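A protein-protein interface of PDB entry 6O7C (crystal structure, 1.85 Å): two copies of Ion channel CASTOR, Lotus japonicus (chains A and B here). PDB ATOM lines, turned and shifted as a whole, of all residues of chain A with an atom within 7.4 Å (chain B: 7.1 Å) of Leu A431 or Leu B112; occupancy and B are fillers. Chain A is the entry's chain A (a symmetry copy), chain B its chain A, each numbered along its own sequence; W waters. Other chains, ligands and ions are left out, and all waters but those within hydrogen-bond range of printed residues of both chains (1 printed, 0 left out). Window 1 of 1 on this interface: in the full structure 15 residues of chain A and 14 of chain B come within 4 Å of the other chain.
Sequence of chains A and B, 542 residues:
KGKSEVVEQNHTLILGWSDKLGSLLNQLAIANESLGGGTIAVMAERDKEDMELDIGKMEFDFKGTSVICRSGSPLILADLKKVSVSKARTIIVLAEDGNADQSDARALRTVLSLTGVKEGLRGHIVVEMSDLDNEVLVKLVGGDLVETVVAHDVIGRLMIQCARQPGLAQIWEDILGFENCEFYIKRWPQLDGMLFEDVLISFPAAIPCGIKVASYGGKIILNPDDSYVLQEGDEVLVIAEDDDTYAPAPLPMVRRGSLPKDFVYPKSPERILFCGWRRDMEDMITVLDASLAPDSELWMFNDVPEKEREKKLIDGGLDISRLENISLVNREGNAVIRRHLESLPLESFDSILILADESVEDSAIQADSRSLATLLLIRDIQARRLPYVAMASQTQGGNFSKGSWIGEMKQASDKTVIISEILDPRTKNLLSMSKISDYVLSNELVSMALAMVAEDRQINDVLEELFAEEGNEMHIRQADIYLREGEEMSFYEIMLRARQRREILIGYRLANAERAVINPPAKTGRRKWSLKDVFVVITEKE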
ATOM      1  N   LEU A 372      20.836  21.982 -34.258  1.00  0.00           N
ATOM      2  CA  LEU A 372      21.938  21.627 -33.336  1.00  0.00           C
ATOM      3  C   LEU A 372      22.063  20.115 -33.131  1.00  0.00           C
ATOM      4  O   LEU A 372      23.180  19.584 -32.946  1.00  0.00           O
ATOM      5  CB  LEU A 372      21.747  22.290 -31.961  1.00  0.00           C
ATOM      6  CG  LEU A 372      21.991  23.805 -32.038  1.00  0.00           C
ATOM      7  CD1 LEU A 372      21.603  24.589 -30.791  1.00  0.00           C
ATOM      8  CD2 LEU A 372      23.469  24.120 -32.387  1.00  0.00           C
ATOM      9  N   LEU A 375      23.833  18.738 -36.126  1.00  0.00           N
ATOM     10  CA  LEU A 375      25.259  19.081 -36.013  1.00  0.00           C
ATOM     11  C   LEU A 375      26.023  18.059 -35.172  1.00  0.00           C
ATOM     12  O   LEU A 375      27.029  17.455 -35.612  1.00  0.00           O
ATOM     13  CB  LEU A 375      25.388  20.459 -35.370  1.00  0.00           C
ATOM     14  CG  LEU A 375      26.831  20.941 -35.121  1.00  0.00           C
ATOM     15  CD1 LEU A 375      27.642  21.003 -36.456  1.00  0.00           C
ATOM     16  CD2 LEU A 375      26.680  22.383 -34.564  1.00  0.00           C
ATOM     17  N   ILE A 422      20.931  29.354 -37.667  1.00  0.00           N
ATOM     18  CA  ILE A 422      20.273  29.549 -36.370  1.00  0.00           C
ATOM     19  C   ILE A 422      19.302  30.725 -36.468  1.00  0.00           C
ATOM     20  O   ILE A 422      19.693  31.850 -36.812  1.00  0.00           O
ATOM     21  CB  ILE A 422      21.286  29.780 -35.250  1.00  0.00           C
ATOM     22  CG1 ILE A 422      22.086  28.495 -35.037  1.00  0.00           C
ATOM     23  CG2 ILE A 422      20.516  30.302 -33.934  1.00  0.00           C
ATOM     24  CD1 ILE A 422      21.265  27.270 -34.529  1.00  0.00           C
ATOM     25  N   PRO A 425      18.551  35.118 -32.711  1.00  0.00           N
ATOM     26  CA  PRO A 425      19.883  35.632 -32.297  1.00  0.00           C
ATOM     27  C   PRO A 425      20.215  35.306 -30.830  1.00  0.00           C
ATOM     28  O   PRO A 425      21.395  35.263 -30.476  1.00  0.00           O
ATOM     29  CB  PRO A 425      19.794  37.158 -32.512  1.00  0.00           C
ATOM     30  CG  PRO A 425      18.656  37.294 -33.593  1.00  0.00           C
ATOM     31  CD  PRO A 425      17.675  36.197 -33.193  1.00  0.00           C
ATOM     32  N   ARG A 426      19.224  35.154 -29.957  1.00  0.00           N
ATOM     33  CA  ARG A 426      19.569  34.878 -28.561  1.00  0.00           C
ATOM     34  C   ARG A 426      20.287  33.524 -28.417  1.00  0.00           C
ATOM     35  O   ARG A 426      21.189  33.363 -27.579  1.00  0.00           O
ATOM     36  CB  ARG A 426      18.330  34.917 -27.684  1.00  0.00           C
ATOM     37  CG  ARG A 426      18.744  34.840 -26.205  1.00  0.00           C
ATOM     38  CD  ARG A 426      17.519  34.722 -25.293  1.00  0.00           C
ATOM     39  NE  ARG A 426      16.616  35.862 -25.448  1.00  0.00           N
ATOM     40  CZ  ARG A 426      16.702  37.007 -24.775  1.00  0.00           C
ATOM     41  NH1 ARG A 426      17.664  37.212 -23.890  1.00  0.00           N
ATOM     42  NH2 ARG A 426      15.813  37.962 -25.016  1.00  0.00           N
ATOM     43  N   THR A 427      19.876  32.532 -29.202  1.00  0.00           N
ATOM     44  CA  THR A 427      20.535  31.232 -29.198  1.00  0.00           C
ATOM     45  C   THR A 427      21.966  31.323 -29.717  1.00  0.00           C
ATOM     46  O   THR A 427      22.886  30.764 -29.124  1.00  0.00           O
ATOM     47  CB  THR A 427      19.667  30.260 -30.006  1.00  0.00           C
ATOM     48  OG1 THR A 427      18.387  30.165 -29.297  1.00  0.00           O
ATOM     49  CG2 THR A 427      20.303  28.894 -30.064  1.00  0.00           C
ATOM     50  N   LYS A 428      22.209  32.148 -30.763  1.00  0.00           N
ATOM     51  CA  LYS A 428      23.607  32.381 -31.143  1.00  0.00           C
ATOM     52  C   LYS A 428      24.390  33.029 -30.000  1.00  0.00           C
ATOM     53  O   LYS A 428      25.508  32.611 -29.660  1.00  0.00           O
ATOM     54  CB  LYS A 428      23.658  33.246 -32.422  1.00  0.00           C
ATOM     55  CG  LYS A 428      25.083  33.467 -33.020  1.00  0.00           C
ATOM     56  CD  LYS A 428      25.649  34.800 -32.453  1.00  0.00           C
ATOM     57  CE  LYS A 428      26.924  35.279 -33.160  1.00  0.00           C
ATOM     58  NZ  LYS A 428      27.373  36.577 -32.519  1.00  0.00           N
ATOM     59  N   ASN A 429      23.825  34.050 -29.363  1.00  0.00           N
ATOM     60  CA  ASN A 429      24.643  34.667 -28.337  1.00  0.00           C
ATOM     61  C   ASN A 429      24.886  33.705 -27.199  1.00  0.00           C
ATOM     62  O   ASN A 429      25.949  33.748 -26.548  1.00  0.00           O
ATOM     63  CB  ASN A 429      23.985  35.931 -27.818  1.00  0.00           C
ATOM     64  CG  ASN A 429      24.074  37.050 -28.811  1.00  0.00           C
ATOM     65  OD1 ASN A 429      25.119  37.222 -29.473  1.00  0.00           O
ATOM     66  ND2 ASN A 429      22.981  37.801 -28.959  1.00  0.00           N
ATOM     67  N   LEU A 430      23.918  32.830 -26.944  1.00  0.00           N
ATOM     68  CA  LEU A 430      24.060  31.911 -25.804  1.00  0.00           C
ATOM     69  C   LEU A 430      25.148  30.879 -26.062  1.00  0.00           C
ATOM     70  O   LEU A 430      25.759  30.351 -25.099  1.00  0.00           O
ATOM     71  CB  LEU A 430      22.734  31.210 -25.511  1.00  0.00           C
ATOM     72  CG  LEU A 430      21.725  32.062 -24.767  1.00  0.00           C
ATOM     73  CD1 LEU A 430      20.431  31.329 -24.682  1.00  0.00           C
ATOM     74  CD2 LEU A 430      22.226  32.310 -23.340  1.00  0.00           C
ATOM     75  N   LEU A 431      25.374  30.570 -27.327  1.00  0.00           N
ATOM     76  CA  LEU A 431      26.377  29.598 -27.754  1.00  0.00           C
ATOM     77  C   LEU A 431      27.788  30.150 -27.792  1.00  0.00           C
ATOM     78  O   LEU A 431      28.701  29.402 -28.153  1.00  0.00           O
ATOM     79  CB  LEU A 431      26.053  29.091 -29.156  1.00  0.00           C
ATOM     80  CG  LEU A 431      24.832  28.196 -29.134  1.00  0.00           C
ATOM     81  CD1 LEU A 431      24.427  28.000 -30.534  1.00  0.00           C
ATOM     82  CD2 LEU A 431      25.222  26.846 -28.424  1.00  0.00           C
ATOM     83  N   SER A 432      27.961  31.434 -27.475  1.00  0.00           N
ATOM     84  CA  SER A 432      29.139  32.161 -27.915  1.00  0.00           C
ATOM     85  C   SER A 432      30.399  31.630 -27.249  1.00  0.00           C
ATOM     86  O   SER A 432      31.459  31.600 -27.878  1.00  0.00           O
ATOM     87  CB  SER A 432      28.965  33.647 -27.630  1.00  0.00           C
ATOM     88  OG  SER A 432      29.010  33.867 -26.226  1.00  0.00           O
ATOM     89  N   MET A 433      30.324  31.189 -25.998  1.00  0.00           N
ATOM     90  CA  MET A 433      31.540  30.655 -25.379  1.00  0.00           C
ATOM     91  C   MET A 433      31.636  29.140 -25.514  1.00  0.00           C
ATOM     92  O   MET A 433      32.507  28.519 -24.885  1.00  0.00           O
ATOM     93  CB  MET A 433      31.680  31.068 -23.900  1.00  0.00           C
ATOM     94  CG  MET A 433      30.840  30.335 -22.829  1.00  0.00           C
ATOM     95  SD  MET A 433      31.182  30.855 -21.091  1.00  0.00           S
ATOM     96  CE  MET A 433      32.666  29.938 -20.622  1.00  0.00           C
ATOM     97  N   SER A 434      30.765  28.544 -26.316  1.00  0.00           N
ATOM     98  CA  SER A 434      30.827  27.137 -26.659  1.00  0.00           C
ATOM     99  C   SER A 434      31.666  26.944 -27.915  1.00  0.00           C
ATOM    100  O   SER A 434      31.708  27.820 -28.790  1.00  0.00           O
ATOM    101  CB  SER A 434      29.415  26.621 -26.904  1.00  0.00           C
ATOM    102  OG  SER A 434      29.498  25.303 -27.383  1.00  0.00           O
ATOM    103  N   LYS A 435      32.299  25.770 -28.028  1.00  0.00           N
ATOM    104  CA  LYS A 435      32.950  25.412 -29.295  1.00  0.00           C
ATOM    105  C   LYS A 435      31.947  25.377 -30.449  1.00  0.00           C
ATOM    106  O   LYS A 435      32.268  25.742 -31.596  1.00  0.00           O
ATOM    107  CB  LYS A 435      33.659  24.061 -29.160  1.00  0.00           C
ATOM    108  CG  LYS A 435      34.443  23.592 -30.407  1.00  0.00           C
ATOM    109  CD  LYS A 435      33.713  22.517 -31.238  1.00  0.00           C
ATOM    110  CE  LYS A 435      33.677  21.150 -30.531  1.00  0.00           C
ATOM    111  NZ  LYS A 435      33.032  20.111 -31.391  1.00  0.00           N
ATOM    112  N   ILE A 436      30.722  24.935 -30.157  1.00  0.00           N
ATOM    113  CA  ILE A 436      29.676  24.850 -31.170  1.00  0.00           C
ATOM    114  C   ILE A 436      29.520  26.151 -31.925  1.00  0.00           C
ATOM    115  O   ILE A 436      29.124  26.142 -33.094  1.00  0.00           O
ATOM    116  CB  ILE A 436      28.369  24.422 -30.465  1.00  0.00           C
ATOM    117  CG1 ILE A 436      28.440  22.931 -30.173  1.00  0.00           C
ATOM    118  CG2 ILE A 436      27.085  24.879 -31.197  1.00  0.00           C
ATOM    119  CD1 ILE A 436      27.546  22.591 -29.043  1.00  0.00           C
ATOM    120  N   SER A 437      29.847  27.289 -31.285  1.00  0.00           N
ATOM    121  CA  SER A 437      29.686  28.610 -31.893  1.00  0.00           C
ATOM    122  C   SER A 437      30.434  28.768 -33.227  1.00  0.00           C
ATOM    123  O   SER A 437      30.082  29.670 -33.985  1.00  0.00           O
ATOM    124  CB  SER A 437      30.172  29.689 -30.930  1.00  0.00           C
ATOM    125  OG  SER A 437      31.567  29.475 -30.695  1.00  0.00           O
ATOM    126  N   ASP A 438      31.458  27.939 -33.527  1.00  0.00           N
ATOM    127  CA  ASP A 438      32.145  28.081 -34.825  1.00  0.00           C
ATOM    128  C   ASP A 438      31.316  27.532 -35.958  1.00  0.00           C
ATOM    129  O   ASP A 438      31.585  27.844 -37.127  1.00  0.00           O
ATOM    130  CB  ASP A 438      33.502  27.360 -34.850  1.00  0.00           C
ATOM    131  CG  ASP A 438      34.547  28.011 -33.934  1.00  0.00           C
ATOM    132  OD1 ASP A 438      34.481  29.248 -33.731  1.00  0.00           O
ATOM    133  OD2 ASP A 438      35.405  27.269 -33.399  1.00  0.00           O
ATOM    134  N   VAL A 440      27.965  27.981 -36.594  1.00  0.00           N
ATOM    135  CA  VAL A 440      26.648  28.646 -36.586  1.00  0.00           C
ATOM    136  C   VAL A 440      26.703  30.001 -37.299  1.00  0.00           C
ATOM    137  O   VAL A 440      27.657  30.763 -37.128  1.00  0.00           O
ATOM    138  CB  VAL A 440      26.127  28.838 -35.136  1.00  0.00           C
ATOM    139  CG1 VAL A 440      25.953  27.482 -34.416  1.00  0.00           C
ATOM    140  CG2 VAL A 440      27.051  29.705 -34.344  1.00  0.00           C
ATOM    141  N   PRO B  74      14.999  32.727 -16.989  1.00  0.00           N
ATOM    142  CA  PRO B  74      16.363  32.257 -16.699  1.00  0.00           C
ATOM    143  C   PRO B  74      17.361  32.624 -17.809  1.00  0.00           C
ATOM    144  O   PRO B  74      18.573  32.482 -17.600  1.00  0.00           O
ATOM    145  CB  PRO B  74      16.187  30.730 -16.557  1.00  0.00           C
ATOM    146  CG  PRO B  74      15.061  30.418 -17.468  1.00  0.00           C
ATOM    147  CD  PRO B  74      14.101  31.627 -17.377  1.00  0.00           C
ATOM    148  N   LEU B  75      16.912  33.167 -18.949  1.00  0.00           N
ATOM    149  CA  LEU B  75      17.842  33.618 -19.994  1.00  0.00           C
ATOM    150  C   LEU B  75      18.284  35.059 -19.819  1.00  0.00           C
ATOM    151  O   LEU B  75      19.078  35.564 -20.627  1.00  0.00           O
ATOM    152  CB  LEU B  75      17.197  33.497 -21.384  1.00  0.00           C
ATOM    153  CG  LEU B  75      16.521  32.147 -21.623  1.00  0.00           C
ATOM    154  CD1 LEU B  75      16.075  32.058 -23.090  1.00  0.00           C
ATOM    155  CD2 LEU B  75      17.383  30.932 -21.291  1.00  0.00           C
ATOM    156  N   ARG B 106      14.322  24.385 -24.115  1.00  0.00           N
ATOM    157  CA  ARG B 106      14.420  25.380 -23.057  1.00  0.00           C
ATOM    158  C   ARG B 106      15.510  25.016 -22.033  1.00  0.00           C
ATOM    159  O   ARG B 106      16.263  25.900 -21.591  1.00  0.00           O
ATOM    160  CB  ARG B 106      13.039  25.515 -22.393  1.00  0.00           C
ATOM    161  CG  ARG B 106      12.914  26.554 -21.270  1.00  0.00           C
ATOM    162  CD  ARG B 106      12.552  25.878 -19.986  1.00  0.00           C
ATOM    163  NE  ARG B 106      12.461  26.726 -18.797  1.00  0.00           N
ATOM    164  CZ  ARG B 106      12.596  26.252 -17.539  1.00  0.00           C
ATOM    165  NH1 ARG B 106      12.549  27.060 -16.497  1.00  0.00           N
ATOM    166  NH2 ARG B 106      12.836  24.975 -17.319  1.00  0.00           N
ATOM    167  N   ALA B 107      15.635  23.748 -21.692  1.00  0.00           N
ATOM    168  CA  ALA B 107      16.688  23.321 -20.746  1.00  0.00           C
ATOM    169  C   ALA B 107      18.068  23.665 -21.269  1.00  0.00           C
ATOM    170  O   ALA B 107      18.910  24.202 -20.529  1.00  0.00           O
ATOM    171  CB  ALA B 107      16.586  21.803 -20.481  1.00  0.00           C
ATOM    172  N   LEU B 108      18.296  23.446 -22.564  1.00  0.00           N
ATOM    173  CA  LEU B 108      19.598  23.740 -23.157  1.00  0.00           C
ATOM    174  C   LEU B 108      19.904  25.240 -23.121  1.00  0.00           C
ATOM    175  O   LEU B 108      21.012  25.670 -22.763  1.00  0.00           O
ATOM    176  CB  LEU B 108      19.603  23.226 -24.610  1.00  0.00           C
ATOM    177  CG  LEU B 108      20.862  23.585 -25.396  1.00  0.00           C
ATOM    178  CD1 LEU B 108      22.170  23.009 -24.797  1.00  0.00           C
ATOM    179  CD2 LEU B 108      20.680  23.152 -26.850  1.00  0.00           C
ATOM    180  N   ARG B 109      18.943  26.057 -23.527  1.00  0.00           N
ATOM    181  CA  ARG B 109      19.148  27.496 -23.436  1.00  0.00           C
ATOM    182  C   ARG B 109      19.404  27.953 -22.006  1.00  0.00           C
ATOM    183  O   ARG B 109      20.265  28.822 -21.750  1.00  0.00           O
ATOM    184  CB  ARG B 109      17.926  28.175 -24.032  1.00  0.00           C
ATOM    185  CG  ARG B 109      17.747  27.805 -25.501  1.00  0.00           C
ATOM    186  CD  ARG B 109      16.442  28.470 -26.014  1.00  0.00           C
ATOM    187  NE  ARG B 109      16.660  29.857 -26.171  1.00  0.00           N
ATOM    188  CZ  ARG B 109      15.742  30.746 -26.540  1.00  0.00           C
ATOM    189  NH1 ARG B 109      14.483  30.380 -26.718  1.00  0.00           N
ATOM    190  NH2 ARG B 109      16.096  31.993 -26.743  1.00  0.00           N
ATOM    191  N   THR B 110      18.641  27.413 -21.051  1.00  0.00           N
ATOM    192  CA  THR B 110      18.883  27.772 -19.658  1.00  0.00           C
ATOM    193  C   THR B 110      20.298  27.404 -19.227  1.00  0.00           C
ATOM    194  O   THR B 110      20.947  28.171 -18.516  1.00  0.00           O
ATOM    195  CB  THR B 110      17.806  27.116 -18.774  1.00  0.00           C
ATOM    196  OG1 THR B 110      16.510  27.604 -19.177  1.00  0.00           O
ATOM    197  CG2 THR B 110      18.004  27.412 -17.314  1.00  0.00           C
ATOM    198  N   VAL B 111      20.768  26.212 -19.586  1.00  0.00           N
ATOM    199  CA  VAL B 111      22.099  25.806 -19.148  1.00  0.00           C
ATOM    200  C   VAL B 111      23.127  26.728 -19.756  1.00  0.00           C
ATOM    201  O   VAL B 111      24.043  27.187 -19.071  1.00  0.00           O
ATOM    202  CB  VAL B 111      22.352  24.324 -19.506  1.00  0.00           C
ATOM    203  CG1 VAL B 111      23.749  23.979 -19.337  1.00  0.00           C
ATOM    204  CG2 VAL B 111      21.530  23.429 -18.615  1.00  0.00           C
ATOM    205  N   LEU B 112      22.959  27.084 -21.022  1.00  0.00           N
ATOM    206  CA  LEU B 112      23.907  28.036 -21.631  1.00  0.00           C
ATOM    207  C   LEU B 112      23.873  29.388 -20.921  1.00  0.00           C
ATOM    208  O   LEU B 112      24.912  30.039 -20.695  1.00  0.00           O
ATOM    209  CB  LEU B 112      23.560  28.217 -23.101  1.00  0.00           C
ATOM    210  CG  LEU B 112      23.860  26.990 -23.971  1.00  0.00           C
ATOM    211  CD1 LEU B 112      23.194  27.148 -25.344  1.00  0.00           C
ATOM    212  CD2 LEU B 112      25.412  26.809 -24.159  1.00  0.00           C
ATOM    213  N   SER B 113      22.680  29.848 -20.576  1.00  0.00           N
ATOM    214  CA  SER B 113      22.556  31.110 -19.876  1.00  0.00           C
ATOM    215  C   SER B 113      23.288  31.046 -18.528  1.00  0.00           C
ATOM    216  O   SER B 113      24.035  31.973 -18.176  1.00  0.00           O
ATOM    217  CB  SER B 113      21.067  31.427 -19.662  1.00  0.00           C
ATOM    218  OG  SER B 113      21.037  32.637 -18.884  1.00  0.00           O
ATOM    219  N   LEU B 114      23.077  29.964 -17.786  1.00  0.00           N
ATOM    220  CA  LEU B 114      23.724  29.797 -16.489  1.00  0.00           C
ATOM    221  C   LEU B 114      25.247  29.709 -16.628  1.00  0.00           C
ATOM    222  O   LEU B 114      25.989  30.270 -15.803  1.00  0.00           O
ATOM    223  CB  LEU B 114      23.194  28.550 -15.804  1.00  0.00           C
ATOM    224  CG  LEU B 114      21.708  28.608 -15.400  1.00  0.00           C
ATOM    225  CD1 LEU B 114      21.243  27.219 -14.959  1.00  0.00           C
ATOM    226  CD2 LEU B 114      21.547  29.613 -14.225  1.00  0.00           C
ATOM    227  N   THR B 115      25.737  28.966 -17.615  1.00  0.00           N
ATOM    228  CA  THR B 115      27.181  28.904 -17.772  1.00  0.00           C
ATOM    229  C   THR B 115      27.736  30.247 -18.227  1.00  0.00           C
ATOM    230  O   THR B 115      28.943  30.469 -18.122  1.00  0.00           O
ATOM    231  CB  THR B 115      27.596  27.817 -18.777  1.00  0.00           C
ATOM    232  OG1 THR B 115      27.064  28.139 -20.044  1.00  0.00           O
ATOM    233  CG2 THR B 115      27.088  26.504 -18.385  1.00  0.00           C
ATOM    234  N   GLY B 116      26.886  31.164 -18.701  1.00  0.00           N
ATOM    235  CA  GLY B 116      27.392  32.482 -19.036  1.00  0.00           C
ATOM    236  C   GLY B 116      27.505  33.488 -17.905  1.00  0.00           C
ATOM    237  O   GLY B 116      28.056  34.567 -18.142  1.00  0.00           O
ATOM    238  N   VAL B 117      27.028  33.177 -16.701  1.00  0.00           N
ATOM    239  CA  VAL B 117      27.038  34.116 -15.573  1.00  0.00           C
ATOM    240  C   VAL B 117      28.474  34.423 -15.175  1.00  0.00           C
ATOM    241  O   VAL B 117      29.235  33.540 -14.775  1.00  0.00           O
ATOM    242  CB  VAL B 117      26.231  33.549 -14.403  1.00  0.00           C
ATOM    243  CG1 VAL B 117      26.402  34.378 -13.139  1.00  0.00           C
ATOM    244  CG2 VAL B 117      24.749  33.499 -14.786  1.00  0.00           C
ATOM    245  N   ILE B 125      24.291  22.537 -11.174  1.00  0.00           N
ATOM    246  CA  ILE B 125      22.986  22.656 -11.850  1.00  0.00           C
ATOM    247  C   ILE B 125      22.419  21.267 -12.050  1.00  0.00           C
ATOM    248  O   ILE B 125      23.061  20.424 -12.694  1.00  0.00           O
ATOM    249  CB  ILE B 125      23.171  23.309 -13.226  1.00  0.00           C
ATOM    250  CG1 ILE B 125      23.951  24.596 -13.107  1.00  0.00           C
ATOM    251  CG2 ILE B 125      21.797  23.488 -13.928  1.00  0.00           C
ATOM    252  CD1 ILE B 125      24.531  25.069 -14.517  1.00  0.00           C
ATOM    253  N   LEU B 137      23.888  16.765 -25.696  1.00  0.00           N
ATOM    254  CA  LEU B 137      24.201  18.156 -26.013  1.00  0.00           C
ATOM    255  C   LEU B 137      24.178  19.004 -24.759  1.00  0.00           C
ATOM    256  O   LEU B 137      25.090  19.795 -24.542  1.00  0.00           O
ATOM    257  CB  LEU B 137      23.209  18.692 -27.047  1.00  0.00           C
ATOM    258  CG  LEU B 137      23.519  20.150 -27.417  1.00  0.00           C
ATOM    259  CD1 LEU B 137      24.971  20.381 -27.845  1.00  0.00           C
ATOM    260  CD2 LEU B 137      22.577  20.373 -28.609  1.00  0.00           C
ATOM    261  N   VAL B 141      27.510  21.075 -23.294  1.00  0.00           N
ATOM    262  CA  VAL B 141      27.689  22.495 -23.039  1.00  0.00           C
ATOM    263  C   VAL B 141      27.735  22.816 -21.554  1.00  0.00           C
ATOM    264  O   VAL B 141      28.252  23.886 -21.194  1.00  0.00           O
ATOM    265  CB  VAL B 141      26.614  23.329 -23.783  1.00  0.00           C
ATOM    266  CG1 VAL B 141      26.693  23.033 -25.298  1.00  0.00           C
ATOM    267  CG2 VAL B 141      25.229  23.073 -23.199  1.00  0.00           C
ATOM    268  N   GLY B 142      27.279  21.908 -20.677  1.00  0.00           N
ATOM    269  CA  GLY B 142      27.200  22.312 -19.277  1.00  0.00           C
ATOM    270  C   GLY B 142      28.504  21.961 -18.564  1.00  0.00           C
ATOM    271  O   GLY B 142      28.799  22.456 -17.455  1.00  0.00           O
HETATM  272  O   HOH W   1      14.501  34.432 -27.333  1.00  0.00           O
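The side-chain sulfur (SD) of Met A433 lies close to the backbone carbonyl oxygen (O) of Thr B115.
O of Pro B74 lies within hydrogen-bond range of OG of Ser B113, at 2.8 Å. O of Val B111 lies close to OG1 of Thr B115 (3.3 Å). The backbone carbonyl oxygen (O) of Leu B112 sits at hydrogen-bond distance from the side-chain hydroxyl (OG1) of Thr B115 (2.9 Å). OG of Ser A434 lies within hydrogen-bond range of N of Ile A436 (3.1 Å).
Among the printed residues, pairs that only touch across the chains: Arg A426 with Arg B109, Thr A427 with Arg B109, Ile A436 with Leu B137, Leu A430 with Leu B112, Leu A430 with Ser B113, Leu A431 with Leu B112, Arg A426 with Leu B75, Leu A430 with Arg B109, Ile A436 with Val B141 and Leu A372 with Leu B137.
Leu B108 touches none of the printed residues of chain A. Of the printed residues of chain A, Thr B115 touches Met A433. Printed residues of chain A within 4 Å of Val B141: Ile A436 (3.9 Å). The nearest residue of chain A that does not touch Leu B112 is Ser A434 (4.9 Å).
Of the 18 printed residues of chain A, 7 touch a printed residue of chain B. Hydrophobic or aromatic side chains of chain A within 4 Å of the printed part of chain B: Leu A372, Leu A430, Leu A431, Met A433 and Ile A436. Hydrophobic or aromatic side chains of chain B within 4 Å of the printed part of chain A: Leu B75, Leu B112, Leu B137 and Val B141. Among the printed residues, no Asp or Glu carboxylate lies within 4 Å of a Lys or Arg side-chain nitrogen of the other chain.
No position is printed for both chains. Of the 11 pairs that touch across the chains among the printed residues, none has its exchanged pair printed and touching as well.
Water W1 bridges the guanidinium group (NH2) of Arg B109 (3.0 Å) and the guanidinium group (NE) of Arg A426 (3.2 Å).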
